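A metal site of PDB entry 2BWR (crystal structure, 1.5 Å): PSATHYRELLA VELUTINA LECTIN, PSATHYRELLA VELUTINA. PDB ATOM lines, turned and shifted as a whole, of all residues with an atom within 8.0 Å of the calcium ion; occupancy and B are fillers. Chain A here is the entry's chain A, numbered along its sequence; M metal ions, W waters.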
ATOM      1  N   ILE A  15     -28.274  25.433   5.224  1.00  0.00           N
ATOM      2  CA  ILE A  15     -27.647  25.236   3.925  1.00  0.00           C
ATOM      3  C   ILE A  15     -26.933  26.534   3.609  1.00  0.00           C
ATOM      4  O   ILE A  15     -27.585  27.555   3.429  1.00  0.00           O
ATOM      5  CB  ILE A  15     -28.702  25.117   2.781  1.00  0.00           C
ATOM      6  CG1 ILE A  15     -29.433  23.790   2.855  1.00  0.00           C
ATOM      7  CG2 ILE A  15     -28.020  25.283   1.422  1.00  0.00           C
ATOM      8  CD1 ILE A  15     -28.564  22.606   2.414  1.00  0.00           C
ATOM      9  N   PRO A  16     -25.604  26.522   3.579  1.00  0.00           N
ATOM     10  CA  PRO A  16     -24.679  25.444   3.850  1.00  0.00           C
ATOM     11  C   PRO A  16     -24.593  25.099   5.307  1.00  0.00           C
ATOM     12  O   PRO A  16     -24.862  25.928   6.185  1.00  0.00           O
ATOM     13  CB  PRO A  16     -23.309  26.019   3.493  1.00  0.00           C
ATOM     14  CG  PRO A  16     -23.503  27.461   3.403  1.00  0.00           C
ATOM     15  CD  PRO A  16     -24.923  27.783   3.228  1.00  0.00           C
ATOM     16  N   GLY A  17     -24.074  23.906   5.590  1.00  0.00           N
ATOM     17  CA  GLY A  17     -23.877  23.503   6.975  1.00  0.00           C
ATOM     18  C   GLY A  17     -23.235  22.147   7.102  1.00  0.00           C
ATOM     19  O   GLY A  17     -23.139  21.424   6.146  1.00  0.00           O
ATOM     20  N   VAL A  18     -22.830  21.847   8.349  1.00  0.00           N
ATOM     21  CA  VAL A  18     -22.278  20.556   8.751  1.00  0.00           C
ATOM     22  C   VAL A  18     -23.148  20.018   9.881  1.00  0.00           C
ATOM     23  O   VAL A  18     -22.853  20.093  11.057  1.00  0.00           O
ATOM     24  CB  VAL A  18     -20.766  20.687   9.162  1.00  0.00           C
ATOM     25  CG1 VAL A  18     -19.941  20.868   7.926  1.00  0.00           C
ATOM     26  CG2 VAL A  18     -20.522  21.852  10.118  1.00  0.00           C
ATOM     27  N   SER A 288     -31.844  21.538  -1.325  1.00  0.00           N
ATOM     28  CA  SER A 288     -30.893  22.071  -2.312  1.00  0.00           C
ATOM     29  C   SER A 288     -29.726  21.154  -2.505  1.00  0.00           C
ATOM     30  O   SER A 288     -29.002  20.906  -1.538  1.00  0.00           O
ATOM     31  CB  SER A 288     -30.341  23.413  -1.903  1.00  0.00           C
ATOM     32  OG  SER A 288     -31.388  24.313  -1.631  1.00  0.00           O
ATOM     33  N   LEU A 289     -29.561  20.651  -3.711  1.00  0.00           N
ATOM     34  CA  LEU A 289     -28.463  19.735  -4.046  1.00  0.00           C
ATOM     35  C   LEU A 289     -27.378  20.365  -4.906  1.00  0.00           C
ATOM     36  O   LEU A 289     -26.412  19.680  -5.265  1.00  0.00           O
ATOM     37  CB  LEU A 289     -29.060  18.552  -4.778  1.00  0.00           C
ATOM     38  CG  LEU A 289     -30.178  17.811  -4.092  1.00  0.00           C
ATOM     39  CD1 LEU A 289     -30.651  16.640  -4.924  1.00  0.00           C
ATOM     40  CD2 LEU A 289     -29.657  17.290  -2.767  1.00  0.00           C
ATOM     41  N   VAL A 342     -29.718  16.467   4.029  1.00  0.00           N
ATOM     42  CA  VAL A 342     -29.180  17.561   4.833  1.00  0.00           C
ATOM     43  C   VAL A 342     -27.710  17.802   4.464  1.00  0.00           C
ATOM     44  O   VAL A 342     -27.003  16.855   4.136  1.00  0.00           O
ATOM     45  CB  VAL A 342     -29.252  17.199   6.354  1.00  0.00           C
ATOM     46  CG1 VAL A 342     -30.618  17.482   6.887  1.00  0.00           C
ATOM     47  CG2 VAL A 342     -28.830  15.769   6.627  1.00  0.00           C
ATOM     48  N   ASP A 343     -27.246  19.034   4.536  1.00  0.00           N
ATOM     49  CA  ASP A 343     -25.835  19.286   4.281  1.00  0.00           C
ATOM     50  C   ASP A 343     -25.031  18.785   5.512  1.00  0.00           C
ATOM     51  O   ASP A 343     -25.225  19.229   6.644  1.00  0.00           O
ATOM     52  CB  ASP A 343     -25.530  20.759   3.972  1.00  0.00           C
ATOM     53  CG  ASP A 343     -24.218  21.017   3.342  1.00  0.00           C
ATOM     54  OD1 ASP A 343     -23.514  20.071   2.972  1.00  0.00           O
ATOM     55  OD2 ASP A 343     -23.904  22.227   3.235  1.00  0.00           O
ATOM     56  N   LEU A 344     -24.095  17.849   5.208  1.00  0.00           N
ATOM     57  CA  LEU A 344     -23.209  17.278   6.214  1.00  0.00           C
ATOM     58  C   LEU A 344     -21.768  17.738   5.975  1.00  0.00           C
ATOM     59  O   LEU A 344     -20.886  17.355   6.777  1.00  0.00           O
ATOM     60  CB  LEU A 344     -23.258  15.743   6.117  1.00  0.00           C
ATOM     61  CG  LEU A 344     -24.607  15.132   6.433  1.00  0.00           C
ATOM     62  CD1 LEU A 344     -24.585  13.656   6.149  1.00  0.00           C
ATOM     63  CD2 LEU A 344     -25.009  15.364   7.900  1.00  0.00           C
ATOM     64  N   THR A 345     -21.516  18.515   4.916  1.00  0.00           N
ATOM     65  CA  THR A 345     -20.155  18.779   4.460  1.00  0.00           C
ATOM     66  C   THR A 345     -19.818  20.257   4.304  1.00  0.00           C
ATOM     67  O   THR A 345     -18.648  20.571   4.109  1.00  0.00           O
ATOM     68  CB  THR A 345     -19.857  18.062   3.136  1.00  0.00           C
ATOM     69  OG1 THR A 345     -20.579  18.699   2.061  1.00  0.00           O
ATOM     70  CG2 THR A 345     -20.204  16.587   3.230  1.00  0.00           C
ATOM     71  N   GLY A 346     -20.810  21.145   4.377  1.00  0.00           N
ATOM     72  CA  GLY A 346     -20.546  22.580   4.389  1.00  0.00           C
ATOM     73  C   GLY A 346     -20.481  23.259   3.041  1.00  0.00           C
ATOM     74  O   GLY A 346     -20.280  24.486   2.982  1.00  0.00           O
ATOM     75  N   ASP A 347     -20.723  22.519   1.965  1.00  0.00           N
ATOM     76  CA  ASP A 347     -20.627  23.060   0.597  1.00  0.00           C
ATOM     77  C   ASP A 347     -21.946  23.667   0.068  1.00  0.00           C
ATOM     78  O   ASP A 347     -22.002  24.190  -1.056  1.00  0.00           O
ATOM     79  CB  ASP A 347     -20.026  22.028  -0.388  1.00  0.00           C
ATOM     80  CG  ASP A 347     -20.971  20.873  -0.732  1.00  0.00           C
ATOM     81  OD1 ASP A 347     -21.876  20.604   0.100  1.00  0.00           O
ATOM     82  OD2 ASP A 347     -20.810  20.278  -1.809  1.00  0.00           O
ATOM     83  N   GLY A 348     -23.003  23.516   0.850  1.00  0.00           N
ATOM     84  CA  GLY A 348     -24.324  23.987   0.405  1.00  0.00           C
ATOM     85  C   GLY A 348     -25.126  23.018  -0.436  1.00  0.00           C
ATOM     86  O   GLY A 348     -26.258  23.347  -0.815  1.00  0.00           O
ATOM     87  N   CYS A 349     -24.586  21.841  -0.705  1.00  0.00           N
ATOM     88  CA  CYS A 349     -25.263  20.821  -1.540  1.00  0.00           C
ATOM     89  C   CYS A 349     -25.630  19.705  -0.598  1.00  0.00           C
ATOM     90  O   CYS A 349     -24.775  19.021  -0.041  1.00  0.00           O
ATOM     91  CB  CYS A 349     -24.332  20.365  -2.661  1.00  0.00           C
ATOM     92  SG  CYS A 349     -23.840  21.813  -3.687  1.00  0.00           S
ATOM     93  N   ALA A 350     -26.907  19.463  -0.380  1.00  0.00           N
ATOM     94  CA  ALA A 350     -27.293  18.504   0.651  1.00  0.00           C
ATOM     95  C   ALA A 350     -26.850  17.077   0.337  1.00  0.00           C
ATOM     96  O   ALA A 350     -26.858  16.630  -0.804  1.00  0.00           O
ATOM     97  CB  ALA A 350     -28.835  18.539   0.889  1.00  0.00           C
ATOM     98  N   ASP A 351     -26.578  16.364   1.421  1.00  0.00           N
ATOM     99  CA  ASP A 351     -26.107  15.000   1.445  1.00  0.00           C
ATOM    100  C   ASP A 351     -27.204  14.092   1.997  1.00  0.00           C
ATOM    101  O   ASP A 351     -28.280  14.557   2.381  1.00  0.00           O
ATOM    102  CB  ASP A 351     -24.861  14.951   2.312  1.00  0.00           C
ATOM    103  CG  ASP A 351     -23.867  16.031   1.911  1.00  0.00           C
ATOM    104  OD1 ASP A 351     -23.386  15.981   0.750  1.00  0.00           O
ATOM    105  OD2 ASP A 351     -23.633  16.977   2.714  1.00  0.00           O
ATOM    106  N   ILE A 352     -26.945  12.791   2.000  1.00  0.00           N
ATOM    107  CA  ILE A 352     -27.922  11.830   2.482  1.00  0.00           C
ATOM    108  C   ILE A 352     -27.386  11.171   3.765  1.00  0.00           C
ATOM    109  O   ILE A 352     -26.238  10.771   3.818  1.00  0.00           O
ATOM    110  CB  ILE A 352     -28.141  10.716   1.417  1.00  0.00           C
ATOM    111  CG1 ILE A 352     -28.791  11.257   0.108  1.00  0.00           C
ATOM    112  CG2 ILE A 352     -28.971   9.603   1.981  1.00  0.00           C
ATOM    113  CD1 ILE A 352     -29.809  12.251   0.443  1.00  0.00           C
ATOM    114  N   CYS A 363     -24.091   9.366   2.372  1.00  0.00           N
ATOM    115  CA  CYS A 363     -23.660   9.404   0.982  1.00  0.00           C
ATOM    116  C   CYS A 363     -23.553  10.853   0.627  1.00  0.00           C
ATOM    117  O   CYS A 363     -24.530  11.573   0.764  1.00  0.00           O
ATOM    118  CB  CYS A 363     -24.705   8.726   0.137  1.00  0.00           C
ATOM    119  SG  CYS A 363     -24.154   8.519  -1.520  1.00  0.00           S
ATOM    120  N   MET A 364     -22.382  11.299   0.200  1.00  0.00           N
ATOM    121  CA  MET A 364     -22.129  12.723   0.071  1.00  0.00           C
ATOM    122  C   MET A 364     -22.305  13.199  -1.384  1.00  0.00           C
ATOM    123  O   MET A 364     -21.932  12.544  -2.335  1.00  0.00           O
ATOM    124  CB  MET A 364     -20.741  13.090   0.576  1.00  0.00           C
ATOM    125  CG  MET A 364     -20.435  12.633   1.997  1.00  0.00           C
ATOM    126  SD  MET A 364     -21.722  13.166   3.194  1.00  0.00           S
ATOM    127  CE  MET A 364     -20.908  12.728   4.741  1.00  0.00           C
ATOM    128  N   ASN A 365     -22.953  14.328  -1.509  1.00  0.00           N
ATOM    129  CA  ASN A 365     -23.088  15.038  -2.781  1.00  0.00           C
ATOM    130  C   ASN A 365     -21.703  15.432  -3.268  1.00  0.00           C
ATOM    131  O   ASN A 365     -20.866  15.974  -2.484  1.00  0.00           O
ATOM    132  CB  ASN A 365     -23.957  16.272  -2.483  1.00  0.00           C
ATOM    133  CG  ASN A 365     -24.580  16.901  -3.710  1.00  0.00           C
ATOM    134  OD1 ASN A 365     -23.967  17.070  -4.737  1.00  0.00           O
ATOM    135  ND2 ASN A 365     -25.844  17.299  -3.563  1.00  0.00           N
ATOM    136  N   LYS A 366     -21.438  15.237  -4.547  1.00  0.00           N
ATOM    137  CA  LYS A 366     -20.185  15.729  -5.140  1.00  0.00           C
ATOM    138  C   LYS A 366     -20.203  17.250  -5.379  1.00  0.00           C
ATOM    139  O   LYS A 366     -19.140  17.859  -5.669  1.00  0.00           O
ATOM    140  CB  LYS A 366     -19.909  14.994  -6.430  1.00  0.00           C
ATOM    141  CG  LYS A 366     -19.636  13.525  -6.204  1.00  0.00           C
ATOM    142  CD  LYS A 366     -19.358  12.832  -7.523  1.00  0.00           C
ATOM    143  CE  LYS A 366     -18.857  11.415  -7.344  1.00  0.00           C
ATOM    144  NZ  LYS A 366     -18.666  10.774  -8.697  1.00  0.00           N
ATOM    145  N   GLY A 367     -21.338  17.890  -5.229  1.00  0.00           N
ATOM    146  CA  GLY A 367     -21.448  19.316  -5.380  1.00  0.00           C
ATOM    147  C   GLY A 367     -22.369  19.750  -6.506  1.00  0.00           C
ATOM    148  O   GLY A 367     -22.641  20.942  -6.619  1.00  0.00           O
ATOM    149  N   PHE A 371     -23.638  11.848  -6.602  1.00  0.00           N
ATOM    150  CA  PHE A 371     -23.292  11.368  -5.280  1.00  0.00           C
ATOM    151  C   PHE A 371     -22.119  10.395  -5.300  1.00  0.00           C
ATOM    152  O   PHE A 371     -21.928   9.665  -6.291  1.00  0.00           O
ATOM    153  CB  PHE A 371     -24.536  10.747  -4.610  1.00  0.00           C
ATOM    154  CG  PHE A 371     -25.476  11.775  -4.078  1.00  0.00           C
ATOM    155  CD1 PHE A 371     -25.441  12.121  -2.735  1.00  0.00           C
ATOM    156  CD2 PHE A 371     -26.333  12.463  -4.897  1.00  0.00           C
ATOM    157  CE1 PHE A 371     -26.265  13.101  -2.260  1.00  0.00           C
ATOM    158  CE2 PHE A 371     -27.153  13.452  -4.409  1.00  0.00           C
ATOM    159  CZ  PHE A 371     -27.118  13.747  -3.081  1.00  0.00           C
HETATM  160 CA    CA M   1     -22.787  18.619   1.150  1.00  0.00          CA
HETATM  161  O   HOH W   1     -21.606  17.940  -0.807  1.00  0.00           O
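The backbone carbonyl oxygen (O) of Val 342 lies within hydrogen-bond range of the backbone NH (N) of Asp 351.
The side-chain sulfur (SG) of Cys 349 sits close to the backbone carbonyl oxygen (O) of Leu 289, 3.7 Å away.
The side-chain carboxylate (OD2) of Asp 343 lies within hydrogen-bond range of the backbone NH (N) of Gly 346, at 3.5 Å.
The backbone NH of Gly 17 sits at hydrogen-bond distance from the side-chain carboxylate of Asp 343 (2.9 Å).
OD2 of Asp 343 lies within hydrogen-bond range of N of Gly 348, 2.9 Å away.
O of Gly 367 sits at hydrogen-bond distance from SG of Cys 349 (3.3 Å).
OD2 of Asp 351 lies close to N of Leu 344, 2.7 Å away.
OD1 of Asp 351 sits close to N of Asn 365, at 2.8 Å.
The nearest printed residue that does not touch the calcium ion is Leu 344 (4.3 Å).
The calcium ion is bound by the backbone carbonyl oxygen (O) of Cys 349 (2.4 Å), water W1 (2.4 Å), the side-chain hydroxyl (OG1) of Thr 345 (2.4 Å), the side-chain carboxylate (OD2) of Asp 351 (2.4 Å), the side-chain carboxylate (OD1) of Asp 347 (2.4 Å), the side-chain carboxylate (OD1) of Asp 343 (2.4 Å) and the side-chain carboxylate (OD1) of Asp 351 (2.7 Å).
Water W1 bridges the side-chain carboxylate of Asp 347 and the backbone carbonyl oxygen of Asn 365.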
